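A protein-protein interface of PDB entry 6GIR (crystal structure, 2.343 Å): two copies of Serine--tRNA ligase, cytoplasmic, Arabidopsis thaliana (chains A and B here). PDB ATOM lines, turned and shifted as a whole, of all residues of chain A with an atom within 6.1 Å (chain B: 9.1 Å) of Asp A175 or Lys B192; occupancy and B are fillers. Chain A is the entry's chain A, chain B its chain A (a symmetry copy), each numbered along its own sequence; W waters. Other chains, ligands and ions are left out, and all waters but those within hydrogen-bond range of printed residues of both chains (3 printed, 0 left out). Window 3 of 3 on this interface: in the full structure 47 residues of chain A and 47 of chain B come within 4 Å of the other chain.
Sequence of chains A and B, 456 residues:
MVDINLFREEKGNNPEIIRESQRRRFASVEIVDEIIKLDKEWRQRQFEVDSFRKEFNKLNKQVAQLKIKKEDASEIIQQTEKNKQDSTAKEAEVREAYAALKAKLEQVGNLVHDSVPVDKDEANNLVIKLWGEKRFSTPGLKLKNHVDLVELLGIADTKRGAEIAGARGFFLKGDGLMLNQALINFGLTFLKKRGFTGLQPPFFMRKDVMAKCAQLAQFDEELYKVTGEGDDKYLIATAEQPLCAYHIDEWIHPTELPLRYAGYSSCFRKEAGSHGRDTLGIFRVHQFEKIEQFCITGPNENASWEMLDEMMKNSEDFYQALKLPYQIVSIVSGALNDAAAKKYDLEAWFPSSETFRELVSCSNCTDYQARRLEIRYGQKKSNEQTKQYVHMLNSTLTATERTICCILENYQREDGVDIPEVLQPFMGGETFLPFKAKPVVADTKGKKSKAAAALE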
ATOM      1  N   GLY A 154       8.027  26.966 -15.042  1.00  0.00           N
ATOM      2  CA  GLY A 154       7.755  26.002 -13.958  1.00  0.00           C
ATOM      3  C   GLY A 154       6.290  25.785 -13.591  1.00  0.00           C
ATOM      4  O   GLY A 154       5.961  25.463 -12.429  1.00  0.00           O
ATOM      5  N   ILE A 155       5.407  25.939 -14.571  1.00  0.00           N
ATOM      6  CA  ILE A 155       3.954  25.948 -14.322  1.00  0.00           C
ATOM      7  C   ILE A 155       3.213  24.683 -14.771  1.00  0.00           C
ATOM      8  O   ILE A 155       1.972  24.618 -14.682  1.00  0.00           O
ATOM      9  CB  ILE A 155       3.279  27.203 -14.922  1.00  0.00           C
ATOM     10  CG1 ILE A 155       3.414  27.258 -16.459  1.00  0.00           C
ATOM     11  CG2 ILE A 155       3.845  28.439 -14.231  1.00  0.00           C
ATOM     12  CD1 ILE A 155       2.609  28.355 -17.098  1.00  0.00           C
ATOM     13  N   LYS A 173       0.939  23.520 -11.969  1.00  0.00           N
ATOM     14  CA  LYS A 173       1.717  23.843 -10.784  1.00  0.00           C
ATOM     15  C   LYS A 173       1.817  25.355 -10.632  1.00  0.00           C
ATOM     16  O   LYS A 173       2.009  26.077 -11.614  1.00  0.00           O
ATOM     17  CB  LYS A 173       3.102  23.198 -10.889  1.00  0.00           C
ATOM     18  CG  LYS A 173       3.927  23.274  -9.617  1.00  0.00           C
ATOM     19  CD  LYS A 173       5.218  22.486  -9.756  1.00  0.00           C
ATOM     20  CE  LYS A 173       6.058  22.584  -8.483  1.00  0.00           C
ATOM     21  NZ  LYS A 173       6.967  21.410  -8.271  1.00  0.00           N
ATOM     22  N   GLY A 174       1.667  25.825  -9.392  1.00  0.00           N
ATOM     23  CA  GLY A 174       1.802  27.231  -9.056  1.00  0.00           C
ATOM     24  C   GLY A 174       0.907  28.091  -9.909  1.00  0.00           C
ATOM     25  O   GLY A 174      -0.315  27.922  -9.888  1.00  0.00           O
ATOM     26  N   ASP A 175       1.527  28.984 -10.681  1.00  0.00           N
ATOM     27  CA  ASP A 175       0.810  29.988 -11.493  1.00  0.00           C
ATOM     28  C   ASP A 175       0.101  29.434 -12.749  1.00  0.00           C
ATOM     29  O   ASP A 175      -0.736  30.122 -13.333  1.00  0.00           O
ATOM     30  CB  ASP A 175       1.770  31.127 -11.871  1.00  0.00           C
ATOM     31  CG  ASP A 175       2.229  31.937 -10.644  1.00  0.00           C
ATOM     32  OD1 ASP A 175       1.358  32.375  -9.856  1.00  0.00           O
ATOM     33  OD2 ASP A 175       3.452  32.138 -10.456  1.00  0.00           O
ATOM     34  N   GLY A 176       0.435  28.209 -13.163  1.00  0.00           N
ATOM     35  CA  GLY A 176      -0.318  27.491 -14.208  1.00  0.00           C
ATOM     36  C   GLY A 176      -1.746  27.219 -13.772  1.00  0.00           C
ATOM     37  O   GLY A 176      -2.688  27.406 -14.533  1.00  0.00           O
ATOM     38  N   LEU A 177      -1.884  26.794 -12.522  1.00  0.00           N
ATOM     39  CA  LEU A 177      -3.173  26.532 -11.890  1.00  0.00           C
ATOM     40  C   LEU A 177      -3.951  27.820 -11.643  1.00  0.00           C
ATOM     41  O   LEU A 177      -5.139  27.847 -11.926  1.00  0.00           O
ATOM     42  CB  LEU A 177      -2.994  25.719 -10.590  1.00  0.00           C
ATOM     43  CG  LEU A 177      -4.240  25.437  -9.736  1.00  0.00           C
ATOM     44  CD1 LEU A 177      -5.394  24.829 -10.519  1.00  0.00           C
ATOM     45  CD2 LEU A 177      -3.842  24.515  -8.610  1.00  0.00           C
ATOM     46  N   MET A 178      -3.316  28.883 -11.140  1.00  0.00           N
ATOM     47  CA  MET A 178      -4.010  30.179 -11.071  1.00  0.00           C
ATOM     48  C   MET A 178      -4.409  30.697 -12.456  1.00  0.00           C
ATOM     49  O   MET A 178      -5.510  31.201 -12.637  1.00  0.00           O
ATOM     50  CB  MET A 178      -3.187  31.244 -10.350  1.00  0.00           C
ATOM     51  CG  MET A 178      -2.833  30.945  -8.892  1.00  0.00           C
ATOM     52  SD  MET A 178      -4.159  30.333  -7.799  1.00  0.00           S
ATOM     53  CE  MET A 178      -3.239  28.950  -7.088  1.00  0.00           C
ATOM     54  N   LEU A 179      -3.533  30.565 -13.446  1.00  0.00           N
ATOM     55  CA  LEU A 179      -3.871  30.933 -14.849  1.00  0.00           C
ATOM     56  C   LEU A 179      -5.031  30.163 -15.439  1.00  0.00           C
ATOM     57  O   LEU A 179      -5.857  30.700 -16.162  1.00  0.00           O
ATOM     58  CB  LEU A 179      -2.700  30.676 -15.775  1.00  0.00           C
ATOM     59  CG  LEU A 179      -1.954  31.859 -16.303  1.00  0.00           C
ATOM     60  CD1 LEU A 179      -0.751  31.326 -17.084  1.00  0.00           C
ATOM     61  CD2 LEU A 179      -2.869  32.668 -17.213  1.00  0.00           C
ATOM     62  N   ASN A 180      -5.030  28.870 -15.190  1.00  0.00           N
ATOM     63  CA  ASN A 180      -6.099  28.028 -15.649  1.00  0.00           C
ATOM     64  C   ASN A 180      -7.421  28.477 -14.990  1.00  0.00           C
ATOM     65  O   ASN A 180      -8.404  28.764 -15.700  1.00  0.00           O
ATOM     66  CB  ASN A 180      -5.758  26.557 -15.358  1.00  0.00           C
ATOM     67  CG  ASN A 180      -6.386  25.593 -16.346  1.00  0.00           C
ATOM     68  OD1 ASN A 180      -6.273  25.768 -17.564  1.00  0.00           O
ATOM     69  ND2 ASN A 180      -7.033  24.559 -15.829  1.00  0.00           N
ATOM     70  N   MET A 427      -6.066  36.895 -10.977  1.00  0.00           N
ATOM     71  CA  MET A 427      -4.878  36.548 -10.158  1.00  0.00           C
ATOM     72  C   MET A 427      -4.463  37.710  -9.247  1.00  0.00           C
ATOM     73  O   MET A 427      -3.255  37.931  -9.014  1.00  0.00           O
ATOM     74  CB  MET A 427      -3.695  36.232 -11.046  1.00  0.00           C
ATOM     75  CG  MET A 427      -4.102  35.623 -12.350  1.00  0.00           C
ATOM     76  SD  MET A 427      -2.934  34.424 -12.983  1.00  0.00           S
ATOM     77  CE  MET A 427      -3.416  34.667 -14.684  1.00  0.00           C
ATOM     78  N   GLU A 430      -1.201  40.007 -10.220  1.00  0.00           N
ATOM     79  CA  GLU A 430       0.148  39.868 -10.775  1.00  0.00           C
ATOM     80  C   GLU A 430       0.116  40.192 -12.297  1.00  0.00           C
ATOM     81  O   GLU A 430      -0.907  40.032 -12.974  1.00  0.00           O
ATOM     82  CB  GLU A 430       0.732  38.466 -10.441  1.00  0.00           C
ATOM     83  CG  GLU A 430       2.229  38.244 -10.688  1.00  0.00           C
ATOM     84  CD  GLU A 430       3.142  39.311 -10.082  1.00  0.00           C
ATOM     85  OE1 GLU A 430       3.243  39.347  -8.837  1.00  0.00           O
ATOM     86  OE2 GLU A 430       3.772  40.099 -10.840  1.00  0.00           O
ATOM     87  N   LEU A 433       4.989  36.610 -14.958  1.00  0.00           N
ATOM     88  CA  LEU A 433       5.464  35.331 -14.462  1.00  0.00           C
ATOM     89  C   LEU A 433       6.909  35.210 -14.939  1.00  0.00           C
ATOM     90  O   LEU A 433       7.170  35.403 -16.128  1.00  0.00           O
ATOM     91  CB  LEU A 433       4.588  34.189 -14.978  1.00  0.00           C
ATOM     92  CG  LEU A 433       3.088  34.224 -14.602  1.00  0.00           C
ATOM     93  CD1 LEU A 433       2.353  32.966 -15.028  1.00  0.00           C
ATOM     94  CD2 LEU A 433       2.891  34.412 -13.108  1.00  0.00           C
ATOM     95  N   PRO A 434       7.868  34.947 -14.012  1.00  0.00           N
ATOM     96  CA  PRO A 434       9.272  34.965 -14.427  1.00  0.00           C
ATOM     97  C   PRO A 434       9.837  33.570 -14.704  1.00  0.00           C
ATOM     98  O   PRO A 434       9.475  32.621 -14.021  1.00  0.00           O
ATOM     99  CB  PRO A 434       9.981  35.592 -13.203  1.00  0.00           C
ATOM    100  CG  PRO A 434       8.939  35.727 -12.126  1.00  0.00           C
ATOM    101  CD  PRO A 434       7.785  34.868 -12.537  1.00  0.00           C
ATOM    102  N   ILE B 184     -13.379  27.069  -4.468  1.00  0.00           N
ATOM    103  CA  ILE B 184     -12.096  26.568  -4.997  1.00  0.00           C
ATOM    104  C   ILE B 184     -11.087  27.693  -5.001  1.00  0.00           C
ATOM    105  O   ILE B 184      -9.956  27.529  -4.561  1.00  0.00           O
ATOM    106  CB  ILE B 184     -12.225  26.008  -6.431  1.00  0.00           C
ATOM    107  CG1 ILE B 184     -12.992  24.697  -6.424  1.00  0.00           C
ATOM    108  CG2 ILE B 184     -10.864  25.779  -7.073  1.00  0.00           C
ATOM    109  CD1 ILE B 184     -13.576  24.319  -7.763  1.00  0.00           C
ATOM    110  N   ASN B 185     -11.499  28.845  -5.505  1.00  0.00           N
ATOM    111  CA  ASN B 185     -10.561  29.927  -5.651  1.00  0.00           C
ATOM    112  C   ASN B 185     -10.216  30.563  -4.294  1.00  0.00           C
ATOM    113  O   ASN B 185      -9.060  30.904  -4.036  1.00  0.00           O
ATOM    114  CB  ASN B 185     -11.053  30.869  -6.749  1.00  0.00           C
ATOM    115  CG  ASN B 185     -10.759  30.295  -8.157  1.00  0.00           C
ATOM    116  OD1 ASN B 185     -11.635  29.739  -8.864  1.00  0.00           O
ATOM    117  ND2 ASN B 185      -9.477  30.407  -8.555  1.00  0.00           N
ATOM    118  N   PHE B 186     -11.190  30.645  -3.401  1.00  0.00           N
ATOM    119  CA  PHE B 186     -10.923  31.100  -2.041  1.00  0.00           C
ATOM    120  C   PHE B 186      -9.969  30.121  -1.334  1.00  0.00           C
ATOM    121  O   PHE B 186      -9.003  30.548  -0.712  1.00  0.00           O
ATOM    122  CB  PHE B 186     -12.244  31.333  -1.249  1.00  0.00           C
ATOM    123  CG  PHE B 186     -12.039  31.491   0.233  1.00  0.00           C
ATOM    124  CD1 PHE B 186     -11.141  32.442   0.729  1.00  0.00           C
ATOM    125  CD2 PHE B 186     -12.698  30.676   1.129  1.00  0.00           C
ATOM    126  CE1 PHE B 186     -10.910  32.573   2.089  1.00  0.00           C
ATOM    127  CE2 PHE B 186     -12.469  30.801   2.504  1.00  0.00           C
ATOM    128  CZ  PHE B 186     -11.580  31.756   2.979  1.00  0.00           C
ATOM    129  N   GLY B 187     -10.218  28.815  -1.436  1.00  0.00           N
ATOM    130  CA  GLY B 187      -9.294  27.822  -0.870  1.00  0.00           C
ATOM    131  C   GLY B 187      -7.885  27.910  -1.441  1.00  0.00           C
ATOM    132  O   GLY B 187      -6.890  27.877  -0.696  1.00  0.00           O
ATOM    133  N   LEU B 188      -7.775  28.044  -2.760  1.00  0.00           N
ATOM    134  CA  LEU B 188      -6.442  28.145  -3.394  1.00  0.00           C
ATOM    135  C   LEU B 188      -5.658  29.407  -3.016  1.00  0.00           C
ATOM    136  O   LEU B 188      -4.442  29.324  -2.771  1.00  0.00           O
ATOM    137  CB  LEU B 188      -6.530  28.031  -4.925  1.00  0.00           C
ATOM    138  CG  LEU B 188      -6.901  26.659  -5.476  1.00  0.00           C
ATOM    139  CD1 LEU B 188      -7.153  26.726  -6.983  1.00  0.00           C
ATOM    140  CD2 LEU B 188      -5.844  25.633  -5.111  1.00  0.00           C
ATOM    141  N   THR B 189      -6.335  30.566  -2.970  1.00  0.00           N
ATOM    142  CA  THR B 189      -5.680  31.815  -2.537  1.00  0.00           C
ATOM    143  C   THR B 189      -5.410  31.746  -1.028  1.00  0.00           C
ATOM    144  O   THR B 189      -4.319  32.090  -0.582  1.00  0.00           O
ATOM    145  CB  THR B 189      -6.461  33.097  -2.922  1.00  0.00           C
ATOM    146  OG1 THR B 189      -7.758  33.068  -2.344  1.00  0.00           O
ATOM    147  CG2 THR B 189      -6.634  33.181  -4.411  1.00  0.00           C
ATOM    148  N   PHE B 190      -6.376  31.251  -0.258  1.00  0.00           N
ATOM    149  CA  PHE B 190      -6.175  30.993   1.187  1.00  0.00           C
ATOM    150  C   PHE B 190      -4.862  30.247   1.435  1.00  0.00           C
ATOM    151  O   PHE B 190      -4.032  30.718   2.190  1.00  0.00           O
ATOM    152  CB  PHE B 190      -7.388  30.247   1.778  1.00  0.00           C
ATOM    153  CG  PHE B 190      -7.269  29.888   3.252  1.00  0.00           C
ATOM    154  CD1 PHE B 190      -6.640  28.712   3.659  1.00  0.00           C
ATOM    155  CD2 PHE B 190      -7.862  30.704   4.243  1.00  0.00           C
ATOM    156  CE1 PHE B 190      -6.562  28.362   5.013  1.00  0.00           C
ATOM    157  CE2 PHE B 190      -7.790  30.361   5.596  1.00  0.00           C
ATOM    158  CZ  PHE B 190      -7.142  29.182   5.981  1.00  0.00           C
ATOM    159  N   LEU B 191      -4.654  29.120   0.773  1.00  0.00           N
ATOM    160  CA  LEU B 191      -3.441  28.322   1.017  1.00  0.00           C
ATOM    161  C   LEU B 191      -2.187  28.949   0.449  1.00  0.00           C
ATOM    162  O   LEU B 191      -1.109  28.790   1.018  1.00  0.00           O
ATOM    163  CB  LEU B 191      -3.591  26.887   0.474  1.00  0.00           C
ATOM    164  CG  LEU B 191      -4.541  25.993   1.264  1.00  0.00           C
ATOM    165  CD1 LEU B 191      -4.679  24.622   0.585  1.00  0.00           C
ATOM    166  CD2 LEU B 191      -4.084  25.845   2.715  1.00  0.00           C
ATOM    167  N   LYS B 192      -2.316  29.618  -0.692  1.00  0.00           N
ATOM    168  CA  LYS B 192      -1.201  30.370  -1.299  1.00  0.00           C
ATOM    169  C   LYS B 192      -0.668  31.411  -0.307  1.00  0.00           C
ATOM    170  O   LYS B 192       0.526  31.486  -0.076  1.00  0.00           O
ATOM    171  CB  LYS B 192      -1.653  31.028  -2.613  1.00  0.00           C
ATOM    172  CG  LYS B 192      -0.599  31.853  -3.318  1.00  0.00           C
ATOM    173  CD  LYS B 192      -0.987  32.130  -4.773  1.00  0.00           C
ATOM    174  CE  LYS B 192      -0.057  33.145  -5.437  1.00  0.00           C
ATOM    175  NZ  LYS B 192      -0.383  33.325  -6.882  1.00  0.00           N
ATOM    176  N   LYS B 193      -1.561  32.165   0.326  1.00  0.00           N
ATOM    177  CA  LYS B 193      -1.148  33.099   1.368  1.00  0.00           C
ATOM    178  C   LYS B 193      -0.333  32.416   2.452  1.00  0.00           C
ATOM    179  O   LYS B 193       0.646  32.972   2.909  1.00  0.00           O
ATOM    180  CB  LYS B 193      -2.353  33.805   1.982  1.00  0.00           C
ATOM    181  CG  LYS B 193      -2.987  34.872   1.098  1.00  0.00           C
ATOM    182  CD  LYS B 193      -4.415  35.160   1.551  1.00  0.00           C
ATOM    183  CE  LYS B 193      -4.862  36.570   1.197  1.00  0.00           C
ATOM    184  NZ  LYS B 193      -4.578  36.938  -0.216  1.00  0.00           N
ATOM    185  N   ARG B 194      -0.722  31.203   2.840  1.00  0.00           N
ATOM    186  CA  ARG B 194      -0.061  30.456   3.923  1.00  0.00           C
ATOM    187  C   ARG B 194       1.074  29.547   3.488  1.00  0.00           C
ATOM    188  O   ARG B 194       1.402  28.597   4.184  1.00  0.00           O
ATOM    189  CB  ARG B 194      -1.111  29.662   4.697  1.00  0.00           C
ATOM    190  CG  ARG B 194      -2.132  30.563   5.391  1.00  0.00           C
ATOM    191  CD  ARG B 194      -3.319  29.775   5.819  1.00  0.00           C
ATOM    192  NE  ARG B 194      -3.906  30.294   7.048  1.00  0.00           N
ATOM    193  CZ  ARG B 194      -4.724  31.329   7.128  1.00  0.00           C
ATOM    194  NH1 ARG B 194      -5.055  32.026   6.047  1.00  0.00           N
ATOM    195  NH2 ARG B 194      -5.206  31.681   8.311  1.00  0.00           N
ATOM    196  N   GLY B 195       1.696  29.839   2.347  1.00  0.00           N
ATOM    197  CA  GLY B 195       2.976  29.233   1.975  1.00  0.00           C
ATOM    198  C   GLY B 195       2.926  28.025   1.048  1.00  0.00           C
ATOM    199  O   GLY B 195       3.941  27.351   0.874  1.00  0.00           O
ATOM    200  N   PHE B 196       1.762  27.772   0.449  1.00  0.00           N
ATOM    201  CA  PHE B 196       1.523  26.574  -0.341  1.00  0.00           C
ATOM    202  C   PHE B 196       1.669  26.861  -1.852  1.00  0.00           C
ATOM    203  O   PHE B 196       1.291  27.948  -2.329  1.00  0.00           O
ATOM    204  CB  PHE B 196       0.089  26.048  -0.074  1.00  0.00           C
ATOM    205  CG  PHE B 196      -0.054  25.181   1.157  1.00  0.00           C
ATOM    206  CD1 PHE B 196       0.072  25.702   2.439  1.00  0.00           C
ATOM    207  CD2 PHE B 196      -0.349  23.830   1.030  1.00  0.00           C
ATOM    208  CE1 PHE B 196      -0.077  24.884   3.558  1.00  0.00           C
ATOM    209  CE2 PHE B 196      -0.497  23.013   2.135  1.00  0.00           C
ATOM    210  CZ  PHE B 196      -0.374  23.539   3.401  1.00  0.00           C
ATOM    211  N   THR B 197       2.169  25.873  -2.595  1.00  0.00           N
ATOM    212  CA  THR B 197       2.216  25.918  -4.059  1.00  0.00           C
ATOM    213  C   THR B 197       1.125  25.017  -4.642  1.00  0.00           C
ATOM    214  O   THR B 197       1.072  23.840  -4.323  1.00  0.00           O
ATOM    215  CB  THR B 197       3.599  25.431  -4.549  1.00  0.00           C
ATOM    216  OG1 THR B 197       4.608  26.330  -4.078  1.00  0.00           O
ATOM    217  CG2 THR B 197       3.681  25.326  -6.080  1.00  0.00           C
ATOM    218  N   GLY B 198       0.269  25.547  -5.509  1.00  0.00           N
ATOM    219  CA  GLY B 198      -0.796  24.740  -6.139  1.00  0.00           C
ATOM    220  C   GLY B 198      -0.295  23.605  -7.036  1.00  0.00           C
ATOM    221  O   GLY B 198       0.787  23.684  -7.583  1.00  0.00           O
ATOM    222  N   LEU B 199      -1.075  22.535  -7.146  1.00  0.00           N
ATOM    223  CA  LEU B 199      -0.806  21.425  -8.065  1.00  0.00           C
ATOM    224  C   LEU B 199      -2.122  20.781  -8.443  1.00  0.00           C
ATOM    225  O   LEU B 199      -2.809  20.280  -7.579  1.00  0.00           O
ATOM    226  CB  LEU B 199       0.069  20.357  -7.427  1.00  0.00           C
ATOM    227  CG  LEU B 199       1.575  20.394  -7.701  1.00  0.00           C
ATOM    228  CD1 LEU B 199       2.300  19.444  -6.758  1.00  0.00           C
ATOM    229  CD2 LEU B 199       1.897  20.065  -9.148  1.00  0.00           C
ATOM    230  N   ARG B 260       5.020  22.375   0.876  1.00  0.00           N
ATOM    231  CA  ARG B 260       3.602  22.571   1.046  1.00  0.00           C
ATOM    232  C   ARG B 260       2.939  22.677  -0.314  1.00  0.00           C
ATOM    233  O   ARG B 260       3.153  23.653  -1.024  1.00  0.00           O
ATOM    234  CB  ARG B 260       3.352  23.845   1.839  1.00  0.00           C
ATOM    235  CG  ARG B 260       4.011  23.882   3.207  1.00  0.00           C
ATOM    236  CD  ARG B 260       3.572  25.130   3.944  1.00  0.00           C
ATOM    237  NE  ARG B 260       4.111  25.188   5.296  1.00  0.00           N
ATOM    238  CZ  ARG B 260       5.334  25.585   5.632  1.00  0.00           C
ATOM    239  NH1 ARG B 260       6.219  25.978   4.741  1.00  0.00           N
ATOM    240  NH2 ARG B 260       5.688  25.564   6.903  1.00  0.00           N
ATOM    241  N   TYR B 261       2.134  21.670  -0.667  1.00  0.00           N
ATOM    242  CA  TYR B 261       1.344  21.672  -1.890  1.00  0.00           C
ATOM    243  C   TYR B 261      -0.153  21.804  -1.565  1.00  0.00           C
ATOM    244  O   TYR B 261      -0.678  21.143  -0.662  1.00  0.00           O
ATOM    245  CB  TYR B 261       1.571  20.387  -2.721  1.00  0.00           C
ATOM    246  CG  TYR B 261       2.996  20.123  -3.135  1.00  0.00           C
ATOM    247  CD1 TYR B 261       3.674  20.974  -4.003  1.00  0.00           C
ATOM    248  CD2 TYR B 261       3.663  19.007  -2.681  1.00  0.00           C
ATOM    249  CE1 TYR B 261       4.998  20.730  -4.372  1.00  0.00           C
ATOM    250  CE2 TYR B 261       4.985  18.748  -3.037  1.00  0.00           C
ATOM    251  CZ  TYR B 261       5.651  19.603  -3.881  1.00  0.00           C
ATOM    252  OH  TYR B 261       6.959  19.304  -4.209  1.00  0.00           O
ATOM    253  N   ALA B 262      -0.836  22.658  -2.309  1.00  0.00           N
ATOM    254  CA  ALA B 262      -2.272  22.702  -2.317  1.00  0.00           C
ATOM    255  C   ALA B 262      -2.829  21.901  -3.516  1.00  0.00           C
ATOM    256  O   ALA B 262      -2.899  22.395  -4.630  1.00  0.00           O
ATOM    257  CB  ALA B 262      -2.726  24.152  -2.375  1.00  0.00           C
ATOM    258  N   ILE B 291     -10.163  20.432  -2.447  1.00  0.00           N
ATOM    259  CA  ILE B 291      -8.892  21.116  -2.254  1.00  0.00           C
ATOM    260  C   ILE B 291      -8.267  20.447  -1.063  1.00  0.00           C
ATOM    261  O   ILE B 291      -8.912  20.247  -0.048  1.00  0.00           O
ATOM    262  CB  ILE B 291      -9.027  22.615  -1.935  1.00  0.00           C
ATOM    263  CG1 ILE B 291      -9.771  23.372  -3.044  1.00  0.00           C
ATOM    264  CG2 ILE B 291      -7.650  23.233  -1.714  1.00  0.00           C
ATOM    265  CD1 ILE B 291      -8.992  23.474  -4.338  1.00  0.00           C
ATOM    266  N   GLN B 293      -4.596  19.897   1.378  1.00  0.00           N
ATOM    267  CA  GLN B 293      -3.260  20.242   1.810  1.00  0.00           C
ATOM    268  C   GLN B 293      -2.491  18.961   1.838  1.00  0.00           C
ATOM    269  O   GLN B 293      -3.011  17.912   2.204  1.00  0.00           O
ATOM    270  CB  GLN B 293      -3.185  20.864   3.191  1.00  0.00           C
ATOM    271  CG  GLN B 293      -4.021  22.111   3.455  1.00  0.00           C
ATOM    272  CD  GLN B 293      -3.979  22.460   4.934  1.00  0.00           C
ATOM    273  OE1 GLN B 293      -2.977  22.975   5.441  1.00  0.00           O
ATOM    274  NE2 GLN B 293      -5.041  22.123   5.642  1.00  0.00           N
ATOM    275  N   ASN B 314      -4.740  25.550   9.715  1.00  0.00           N
ATOM    276  CA  ASN B 314      -5.129  26.067   8.405  1.00  0.00           C
ATOM    277  C   ASN B 314      -6.570  25.705   8.080  1.00  0.00           C
ATOM    278  O   ASN B 314      -7.327  26.552   7.622  1.00  0.00           O
ATOM    279  CB  ASN B 314      -4.172  25.572   7.315  1.00  0.00           C
ATOM    280  CG  ASN B 314      -2.775  26.152   7.445  1.00  0.00           C
ATOM    281  OD1 ASN B 314      -2.582  27.234   8.015  1.00  0.00           O
ATOM    282  ND2 ASN B 314      -1.779  25.423   6.927  1.00  0.00           N
ATOM    283  N   LEU B 397      -8.910  20.557   2.791  1.00  0.00           N
ATOM    284  CA  LEU B 397      -9.368  21.889   3.087  1.00  0.00           C
ATOM    285  C   LEU B 397     -10.873  21.921   2.792  1.00  0.00           C
ATOM    286  O   LEU B 397     -11.648  22.326   3.653  1.00  0.00           O
ATOM    287  CB  LEU B 397      -8.594  22.930   2.279  1.00  0.00           C
ATOM    288  CG  LEU B 397      -8.690  24.374   2.788  1.00  0.00           C
ATOM    289  CD1 LEU B 397      -7.750  24.591   3.960  1.00  0.00           C
ATOM    290  CD2 LEU B 397      -8.381  25.369   1.682  1.00  0.00           C
HETATM  291  O   HOH W   1       0.370  30.787  -7.802  1.00  0.00           O
HETATM  292  O   HOH W   2       8.068  21.393  -5.610  1.00  0.00           O
HETATM  293  O   HOH W   3      -7.594  32.257 -10.602  1.00  0.00           O
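Hydrophobic or aromatic side chains of chain B that line the printed part of chain A: Leu B199. Among the printed residues, Asp or Glu carboxylates within 4 Å of a Lys or Arg side-chain nitrogen of the other chain: Asp A175 with Lys B192 (3.6 Å).
No position is printed for both chains.
Water W2 lies within hydrogen-bond range of OH of Tyr B261 (2.7 Å) and NZ of Lys A173 (2.9 Å). Water W1 lies within hydrogen-bond range of the side-chain carboxylate of Asp A175 (2.8 Å) and the side-chain amino group of Lys B192 (2.8 Å). Water W3 bridges O of Met A178 (3.1 Å) and ND2 of Asn B185 (3.3 Å).
O of Gly B198 touches CA of Lys A173, at 3.3 Å. CB of Lys A173 touches CD2 of Leu B199, 3.8 Å away. Gly A174 touches Thr B197. Leu A177 touches Gly B198. N of Leu B199 touches CD2 of Leu A177 (3.7 Å). Met A178 touches Lys B192.
O of Gly B198 is in hydrogen-bond range of N of Gly A174, at 2.9 Å. The side-chain carboxylate (OD1) of Asp A175 is in salt-bridge range of the side-chain amino group (NZ) of Lys B192 (3.6 Å).
Gly A174 touches just these residues of chain B: Thr B197 and Gly B198. Of chain B, only Lys B192 (3.6 Å) comes within 4 Å of Asp A175. Met A178 touches one residue of chain B. Printed residues of chain A within 4 Å of Lys B192: Asp A175 and Met A178. Printed residues of chain A within 4 Å of Gly B198: Lys A173 (3.3 Å), Gly A174 (2.9 Å) and Leu A177 (3.9 Å). Printed residues of chain A within 4 Å of Leu B199: Lys A173 and Leu A177.
O of Thr B197 is in hydrogen-bond range of N of Ala B262. The backbone NH (N) of Leu B199 lies within hydrogen-bond range of the backbone carbonyl oxygen (O) of Ala B262 (3.1 Å). The backbone carbonyl oxygen (O) of Arg B260 lies within hydrogen-bond range of the backbone NH (N) of Thr B197 (2.9 Å). The backbone carbonyl oxygen of Ile A155 lies within hydrogen-bond range of the backbone NH of Lys A173 (3.1 Å).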
